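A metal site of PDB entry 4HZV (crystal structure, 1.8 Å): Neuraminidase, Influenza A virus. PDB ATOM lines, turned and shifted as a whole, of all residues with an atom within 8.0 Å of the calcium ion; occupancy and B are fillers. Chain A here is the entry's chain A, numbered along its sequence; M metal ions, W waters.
The calcium ion is bound by the backbone carbonyl oxygen (O) of Asp 213 (2.4 Å), the backbone carbonyl oxygen (O) of Gly 263 (2.4 Å), the side-chain carboxylate (OD2) of Asp 243 (2.5 Å), the backbone carbonyl oxygen (O) of Pro 265 (2.5 Å), the backbone carbonyl oxygen (O) of Gly 217 (2.6 Å) and water W1 (2.6 Å).
Gly 266 touches the calcium ion.
Of the 26 residues printed, 6 come within 4 Å of the calcium ion.
N of Trp 215 sits at hydrogen-bond distance from OD1 of Asp 213, 2.8 Å away.
The side-chain carboxylate of Asp 213 sits at hydrogen-bond distance from the side-chain hydroxyl of Tyr 235 (2.5 Å).
O of Asp 243 lies within hydrogen-bond range of NH2 of Arg 246, 3.0 Å away.
The backbone NH (N) of Gly 266 lies within hydrogen-bond range of the side-chain amide oxygen (OD1) of Asn 214 (3.0 Å).
The backbone carbonyl oxygen (O) of Gly 266 is in hydrogen-bond range of the guanidinium group (NH2) of Arg 212, 3.3 Å away.
O of Ser 218 sits close to N of Asp 243.
The side-chain carboxylate (OD1) of Asp 213 lies within hydrogen-bond range of the backbone NH (N) of Gly 217, at 3.1 Å.
The backbone carbonyl oxygen of Pro 265 sits close to the side-chain amide oxygen of Asn 214 (3.2 Å).
Water W1 bridges O of Pro 245 (2.5 Å) and O of Asn 262 (2.7 Å).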
ATOM      1  N   HIS A 195     -10.286 -27.495  20.832  1.00  0.00           N
ATOM      2  CA  HIS A 195     -10.097 -28.807  21.452  1.00  0.00           C
ATOM      3  C   HIS A 195     -10.436 -28.726  22.937  1.00  0.00           C
ATOM      4  O   HIS A 195     -10.121 -27.733  23.600  1.00  0.00           O
ATOM      5  CB  HIS A 195      -8.687 -29.344  21.219  1.00  0.00           C
ATOM      6  CG  HIS A 195      -8.529 -30.801  21.554  1.00  0.00           C
ATOM      7  ND1 HIS A 195      -8.930 -31.802  20.703  1.00  0.00           N
ATOM      8  CD2 HIS A 195      -8.025 -31.412  22.650  1.00  0.00           C
ATOM      9  CE1 HIS A 195      -8.683 -32.975  21.255  1.00  0.00           C
ATOM     10  NE2 HIS A 195      -8.129 -32.770  22.442  1.00  0.00           N
ATOM     11  N   CYS A 211     -11.213 -25.996  30.946  1.00  0.00           N
ATOM     12  CA  CYS A 211     -10.810 -27.319  30.477  1.00  0.00           C
ATOM     13  C   CYS A 211      -9.391 -27.349  29.912  1.00  0.00           C
ATOM     14  O   CYS A 211      -8.570 -26.478  30.209  1.00  0.00           O
ATOM     15  CB  CYS A 211     -11.824 -27.826  29.450  1.00  0.00           C
ATOM     16  SG  CYS A 211     -13.525 -27.458  29.944  1.00  0.00           S
ATOM     17  N   ARG A 212      -9.113 -28.381  29.133  1.00  0.00           N
ATOM     18  CA  ARG A 212      -7.794 -28.621  28.579  1.00  0.00           C
ATOM     19  C   ARG A 212      -7.887 -28.729  27.065  1.00  0.00           C
ATOM     20  O   ARG A 212      -8.562 -29.603  26.539  1.00  0.00           O
ATOM     21  CB  ARG A 212      -7.229 -29.910  29.172  1.00  0.00           C
ATOM     22  CG  ARG A 212      -6.058 -30.538  28.419  1.00  0.00           C
ATOM     23  CD  ARG A 212      -5.620 -31.820  29.116  1.00  0.00           C
ATOM     24  NE  ARG A 212      -4.667 -32.614  28.341  1.00  0.00           N
ATOM     25  CZ  ARG A 212      -4.081 -33.722  28.770  1.00  0.00           C
ATOM     26  NH1 ARG A 212      -4.312 -34.178  30.000  1.00  0.00           N
ATOM     27  NH2 ARG A 212      -3.239 -34.371  27.980  1.00  0.00           N
ATOM     28  N   ASP A 213      -7.228 -27.816  26.364  1.00  0.00           N
ATOM     29  CA  ASP A 213      -7.070 -27.910  24.913  1.00  0.00           C
ATOM     30  C   ASP A 213      -5.790 -28.698  24.704  1.00  0.00           C
ATOM     31  O   ASP A 213      -4.729 -28.238  25.097  1.00  0.00           O
ATOM     32  CB  ASP A 213      -6.975 -26.503  24.313  1.00  0.00           C
ATOM     33  CG  ASP A 213      -6.731 -26.518  22.805  1.00  0.00           C
ATOM     34  OD1 ASP A 213      -5.973 -27.381  22.317  1.00  0.00           O
ATOM     35  OD2 ASP A 213      -7.315 -25.653  22.109  1.00  0.00           O
ATOM     36  N   ASN A 214      -5.883 -29.882  24.127  1.00  0.00           N
ATOM     37  CA  ASN A 214      -4.718 -30.761  24.051  1.00  0.00           C
ATOM     38  C   ASN A 214      -3.998 -30.648  22.706  1.00  0.00           C
ATOM     39  O   ASN A 214      -3.093 -31.423  22.410  1.00  0.00           O
ATOM     40  CB  ASN A 214      -5.141 -32.211  24.292  1.00  0.00           C
ATOM     41  CG  ASN A 214      -4.002 -33.073  24.778  1.00  0.00           C
ATOM     42  OD1 ASN A 214      -3.311 -32.726  25.735  1.00  0.00           O
ATOM     43  ND2 ASN A 214      -3.795 -34.217  24.127  1.00  0.00           N
ATOM     44  N   TRP A 215      -4.390 -29.663  21.922  1.00  0.00           N
ATOM     45  CA  TRP A 215      -3.985 -29.610  20.525  1.00  0.00           C
ATOM     46  C   TRP A 215      -3.190 -28.336  20.196  1.00  0.00           C
ATOM     47  O   TRP A 215      -1.992 -28.399  19.928  1.00  0.00           O
ATOM     48  CB  TRP A 215      -5.220 -29.734  19.637  1.00  0.00           C
ATOM     49  CG  TRP A 215      -4.967 -29.765  18.170  1.00  0.00           C
ATOM     50  CD1 TRP A 215      -3.772 -30.009  17.542  1.00  0.00           C
ATOM     51  CD2 TRP A 215      -5.932 -29.567  17.129  1.00  0.00           C
ATOM     52  NE1 TRP A 215      -3.935 -29.959  16.178  1.00  0.00           N
ATOM     53  CE2 TRP A 215      -5.255 -29.691  15.895  1.00  0.00           C
ATOM     54  CE3 TRP A 215      -7.296 -29.284  17.124  1.00  0.00           C
ATOM     55  CZ2 TRP A 215      -5.906 -29.556  14.673  1.00  0.00           C
ATOM     56  CZ3 TRP A 215      -7.943 -29.143  15.908  1.00  0.00           C
ATOM     57  CH2 TRP A 215      -7.244 -29.275  14.700  1.00  0.00           C
ATOM     58  N   LYS A 216      -3.857 -27.185  20.243  1.00  0.00           N
ATOM     59  CA  LYS A 216      -3.232 -25.934  19.812  1.00  0.00           C
ATOM     60  C   LYS A 216      -3.182 -24.871  20.913  1.00  0.00           C
ATOM     61  O   LYS A 216      -2.566 -23.822  20.722  1.00  0.00           O
ATOM     62  CB  LYS A 216      -3.991 -25.378  18.604  1.00  0.00           C
ATOM     63  CG  LYS A 216      -4.027 -26.315  17.413  1.00  0.00           C
ATOM     64  CD  LYS A 216      -5.039 -25.844  16.373  1.00  0.00           C
ATOM     65  CE  LYS A 216      -6.443 -25.764  16.957  1.00  0.00           C
ATOM     66  NZ  LYS A 216      -7.455 -25.451  15.906  1.00  0.00           N
ATOM     67  N   GLY A 217      -3.826 -25.133  22.035  1.00  0.00           N
ATOM     68  CA  GLY A 217      -3.968 -24.097  23.051  1.00  0.00           C
ATOM     69  C   GLY A 217      -3.182 -24.291  24.325  1.00  0.00           C
ATOM     70  O   GLY A 217      -3.398 -25.246  25.055  1.00  0.00           O
ATOM     71  N   SER A 218      -2.253 -23.373  24.585  1.00  0.00           N
ATOM     72  CA  SER A 218      -1.546 -23.341  25.867  1.00  0.00           C
ATOM     73  C   SER A 218      -2.389 -22.570  26.877  1.00  0.00           C
ATOM     74  O   SER A 218      -2.165 -22.662  28.089  1.00  0.00           O
ATOM     75  CB  SER A 218      -0.154 -22.710  25.707  1.00  0.00           C
ATOM     76  OG  SER A 218      -0.241 -21.369  25.242  1.00  0.00           O
ATOM     77  N   ASN A 219      -3.356 -21.831  26.361  1.00  0.00           N
ATOM     78  CA  ASN A 219      -4.406 -21.230  27.190  1.00  0.00           C
ATOM     79  C   ASN A 219      -5.557 -22.235  27.329  1.00  0.00           C
ATOM     80  O   ASN A 219      -5.728 -23.115  26.493  1.00  0.00           O
ATOM     81  CB  ASN A 219      -4.897 -19.899  26.585  1.00  0.00           C
ATOM     82  CG  ASN A 219      -5.197 -20.001  25.087  1.00  0.00           C
ATOM     83  OD1 ASN A 219      -4.797 -20.948  24.411  1.00  0.00           O
ATOM     84  ND2 ASN A 219      -5.910 -19.013  24.565  1.00  0.00           N
ATOM     85  N   ARG A 220      -6.326 -22.120  28.413  1.00  0.00           N
ATOM     86  CA  ARG A 220      -7.399 -23.066  28.661  1.00  0.00           C
ATOM     87  C   ARG A 220      -8.743 -22.601  28.085  1.00  0.00           C
ATOM     88  O   ARG A 220      -9.160 -21.473  28.324  1.00  0.00           O
ATOM     89  CB  ARG A 220      -7.550 -23.340  30.154  1.00  0.00           C
ATOM     90  CG  ARG A 220      -6.342 -24.027  30.776  1.00  0.00           C
ATOM     91  CD  ARG A 220      -6.673 -24.571  32.158  1.00  0.00           C
ATOM     92  NE  ARG A 220      -5.548 -25.284  32.750  1.00  0.00           N
ATOM     93  CZ  ARG A 220      -5.170 -26.501  32.376  1.00  0.00           C
ATOM     94  NH1 ARG A 220      -5.823 -27.134  31.405  1.00  0.00           N
ATOM     95  NH2 ARG A 220      -4.132 -27.088  32.956  1.00  0.00           N
ATOM     96  N   PRO A 221      -9.421 -23.492  27.344  1.00  0.00           N
ATOM     97  CA  PRO A 221     -10.768 -23.216  26.837  1.00  0.00           C
ATOM     98  C   PRO A 221     -11.767 -23.270  27.986  1.00  0.00           C
ATOM     99  O   PRO A 221     -11.502 -23.932  28.989  1.00  0.00           O
ATOM    100  CB  PRO A 221     -11.016 -24.378  25.867  1.00  0.00           C
ATOM    101  CG  PRO A 221     -10.183 -25.486  26.388  1.00  0.00           C
ATOM    102  CD  PRO A 221      -8.950 -24.833  26.944  1.00  0.00           C
ATOM    103  N   TYR A 235     -11.665 -18.869  25.360  1.00  0.00           N
ATOM    104  CA  TYR A 235     -10.438 -19.237  26.051  1.00  0.00           C
ATOM    105  C   TYR A 235     -10.175 -18.190  27.128  1.00  0.00           C
ATOM    106  O   TYR A 235     -10.606 -17.033  27.004  1.00  0.00           O
ATOM    107  CB  TYR A 235      -9.264 -19.336  25.087  1.00  0.00           C
ATOM    108  CG  TYR A 235      -9.250 -20.594  24.252  1.00  0.00           C
ATOM    109  CD1 TYR A 235     -10.068 -20.716  23.131  1.00  0.00           C
ATOM    110  CD2 TYR A 235      -8.410 -21.653  24.564  1.00  0.00           C
ATOM    111  CE1 TYR A 235     -10.058 -21.865  22.359  1.00  0.00           C
ATOM    112  CE2 TYR A 235      -8.387 -22.799  23.797  1.00  0.00           C
ATOM    113  CZ  TYR A 235      -9.208 -22.910  22.698  1.00  0.00           C
ATOM    114  OH  TYR A 235      -9.193 -24.052  21.946  1.00  0.00           O
ATOM    115  N   SER A 242      -2.063 -21.122  31.554  1.00  0.00           N
ATOM    116  CA  SER A 242      -2.097 -22.065  32.671  1.00  0.00           C
ATOM    117  C   SER A 242      -2.150 -23.554  32.316  1.00  0.00           C
ATOM    118  O   SER A 242      -2.381 -24.394  33.188  1.00  0.00           O
ATOM    119  CB  SER A 242      -3.238 -21.714  33.640  1.00  0.00           C
ATOM    120  OG  SER A 242      -4.495 -21.867  33.013  1.00  0.00           O
ATOM    121  N   ASP A 243      -1.927 -23.890  31.053  1.00  0.00           N
ATOM    122  CA  ASP A 243      -1.798 -25.301  30.690  1.00  0.00           C
ATOM    123  C   ASP A 243      -0.346 -25.728  30.864  1.00  0.00           C
ATOM    124  O   ASP A 243       0.509 -24.904  31.172  1.00  0.00           O
ATOM    125  CB  ASP A 243      -2.268 -25.538  29.248  1.00  0.00           C
ATOM    126  CG  ASP A 243      -2.756 -26.961  29.005  1.00  0.00           C
ATOM    127  OD1 ASP A 243      -2.595 -27.828  29.892  1.00  0.00           O
ATOM    128  OD2 ASP A 243      -3.310 -27.220  27.920  1.00  0.00           O
ATOM    129  N   THR A 244      -0.078 -27.016  30.678  1.00  0.00           N
ATOM    130  CA  THR A 244       1.279 -27.540  30.667  1.00  0.00           C
ATOM    131  C   THR A 244       1.423 -28.593  29.559  1.00  0.00           C
ATOM    132  O   THR A 244       0.777 -29.641  29.611  1.00  0.00           O
ATOM    133  CB  THR A 244       1.661 -28.196  32.011  1.00  0.00           C
ATOM    134  OG1 THR A 244       1.402 -27.280  33.082  1.00  0.00           O
ATOM    135  CG2 THR A 244       3.138 -28.571  32.023  1.00  0.00           C
ATOM    136  N   PRO A 245       2.289 -28.329  28.576  1.00  0.00           N
ATOM    137  CA  PRO A 245       3.237 -27.206  28.507  1.00  0.00           C
ATOM    138  C   PRO A 245       2.599 -25.861  28.166  1.00  0.00           C
ATOM    139  O   PRO A 245       1.411 -25.792  27.832  1.00  0.00           O
ATOM    140  CB  PRO A 245       4.175 -27.632  27.383  1.00  0.00           C
ATOM    141  CG  PRO A 245       3.331 -28.450  26.487  1.00  0.00           C
ATOM    142  CD  PRO A 245       2.430 -29.230  27.407  1.00  0.00           C
ATOM    143  N   ARG A 246       3.401 -24.805  28.242  1.00  0.00           N
ATOM    144  CA  ARG A 246       2.952 -23.450  27.945  1.00  0.00           C
ATOM    145  C   ARG A 246       4.170 -22.539  27.812  1.00  0.00           C
ATOM    146  O   ARG A 246       5.242 -22.874  28.318  1.00  0.00           O
ATOM    147  CB  ARG A 246       2.060 -22.929  29.067  1.00  0.00           C
ATOM    148  CG  ARG A 246       2.775 -22.832  30.418  1.00  0.00           C
ATOM    149  CD  ARG A 246       1.942 -22.095  31.455  1.00  0.00           C
ATOM    150  NE  ARG A 246       2.688 -21.904  32.707  1.00  0.00           N
ATOM    151  CZ  ARG A 246       2.789 -22.841  33.640  1.00  0.00           C
ATOM    152  NH1 ARG A 246       3.484 -22.599  34.748  1.00  0.00           N
ATOM    153  NH2 ARG A 246       2.203 -24.023  33.464  1.00  0.00           N
ATOM    154  N   SER A 259      -3.949 -20.362  21.758  1.00  0.00           N
ATOM    155  CA  SER A 259      -2.745 -19.546  21.622  1.00  0.00           C
ATOM    156  C   SER A 259      -1.953 -19.891  20.368  1.00  0.00           C
ATOM    157  O   SER A 259      -1.357 -19.012  19.741  1.00  0.00           O
ATOM    158  CB  SER A 259      -1.849 -19.733  22.852  1.00  0.00           C
ATOM    159  OG  SER A 259      -1.213 -21.001  22.819  1.00  0.00           O
ATOM    160  N   VAL A 261       0.674 -21.721  20.432  1.00  0.00           N
ATOM    161  CA  VAL A 261       2.066 -21.878  20.852  1.00  0.00           C
ATOM    162  C   VAL A 261       2.146 -22.854  22.025  1.00  0.00           C
ATOM    163  O   VAL A 261       1.355 -22.766  22.962  1.00  0.00           O
ATOM    164  CB  VAL A 261       2.706 -20.529  21.246  1.00  0.00           C
ATOM    165  CG1 VAL A 261       3.035 -19.705  20.002  1.00  0.00           C
ATOM    166  CG2 VAL A 261       1.777 -19.749  22.161  1.00  0.00           C
ATOM    167  N   ASN A 262       3.096 -23.787  21.954  1.00  0.00           N
ATOM    168  CA  ASN A 262       3.212 -24.850  22.959  1.00  0.00           C
ATOM    169  C   ASN A 262       1.862 -25.509  23.199  1.00  0.00           C
ATOM    170  O   ASN A 262       1.437 -25.740  24.339  1.00  0.00           O
ATOM    171  CB  ASN A 262       3.784 -24.291  24.257  1.00  0.00           C
ATOM    172  CG  ASN A 262       5.175 -23.724  24.070  1.00  0.00           C
ATOM    173  OD1 ASN A 262       6.109 -24.453  23.740  1.00  0.00           O
ATOM    174  ND2 ASN A 262       5.318 -22.418  24.259  1.00  0.00           N
ATOM    175  N   GLY A 263       1.194 -25.834  22.096  1.00  0.00           N
ATOM    176  CA  GLY A 263      -0.201 -26.202  22.116  1.00  0.00           C
ATOM    177  C   GLY A 263      -0.518 -27.571  22.676  1.00  0.00           C
ATOM    178  O   GLY A 263      -1.552 -27.733  23.303  1.00  0.00           O
ATOM    179  N   GLY A 264       0.351 -28.551  22.439  1.00  0.00           N
ATOM    180  CA  GLY A 264       0.095 -29.904  22.897  1.00  0.00           C
ATOM    181  C   GLY A 264       1.276 -30.479  23.656  1.00  0.00           C
ATOM    182  O   GLY A 264       2.400 -30.023  23.467  1.00  0.00           O
ATOM    183  N   PRO A 265       1.024 -31.458  24.542  1.00  0.00           N
ATOM    184  CA  PRO A 265      -0.322 -31.971  24.865  1.00  0.00           C
ATOM    185  C   PRO A 265      -1.023 -31.035  25.836  1.00  0.00           C
ATOM    186  O   PRO A 265      -1.589 -30.029  25.420  1.00  0.00           O
ATOM    187  CB  PRO A 265      -0.034 -33.307  25.557  1.00  0.00           C
ATOM    188  CG  PRO A 265       1.426 -33.596  25.305  1.00  0.00           C
ATOM    189  CD  PRO A 265       2.071 -32.255  25.190  1.00  0.00           C
ATOM    190  N   GLY A 266      -0.997 -31.372  27.126  1.00  0.00           N
ATOM    191  CA  GLY A 266      -1.621 -30.546  28.145  1.00  0.00           C
ATOM    192  C   GLY A 266      -1.717 -31.302  29.454  1.00  0.00           C
ATOM    193  O   GLY A 266      -1.187 -32.395  29.590  1.00  0.00           O
ATOM    194  N   VAL A 267      -2.404 -30.704  30.415  1.00  0.00           N
ATOM    195  CA  VAL A 267      -2.706 -31.383  31.667  1.00  0.00           C
ATOM    196  C   VAL A 267      -4.036 -30.857  32.188  1.00  0.00           C
ATOM    197  O   VAL A 267      -4.375 -29.695  31.986  1.00  0.00           O
ATOM    198  CB  VAL A 267      -1.586 -31.150  32.720  1.00  0.00           C
ATOM    199  CG1 VAL A 267      -1.525 -29.689  33.146  1.00  0.00           C
ATOM    200  CG2 VAL A 267      -1.782 -32.063  33.939  1.00  0.00           C
HETATM  201 CA    CA M   1      -2.465 -27.649  25.566  1.00  0.00          CA
HETATM  202  O   HOH W   1       0.036 -27.090  26.152  1.00  0.00           O
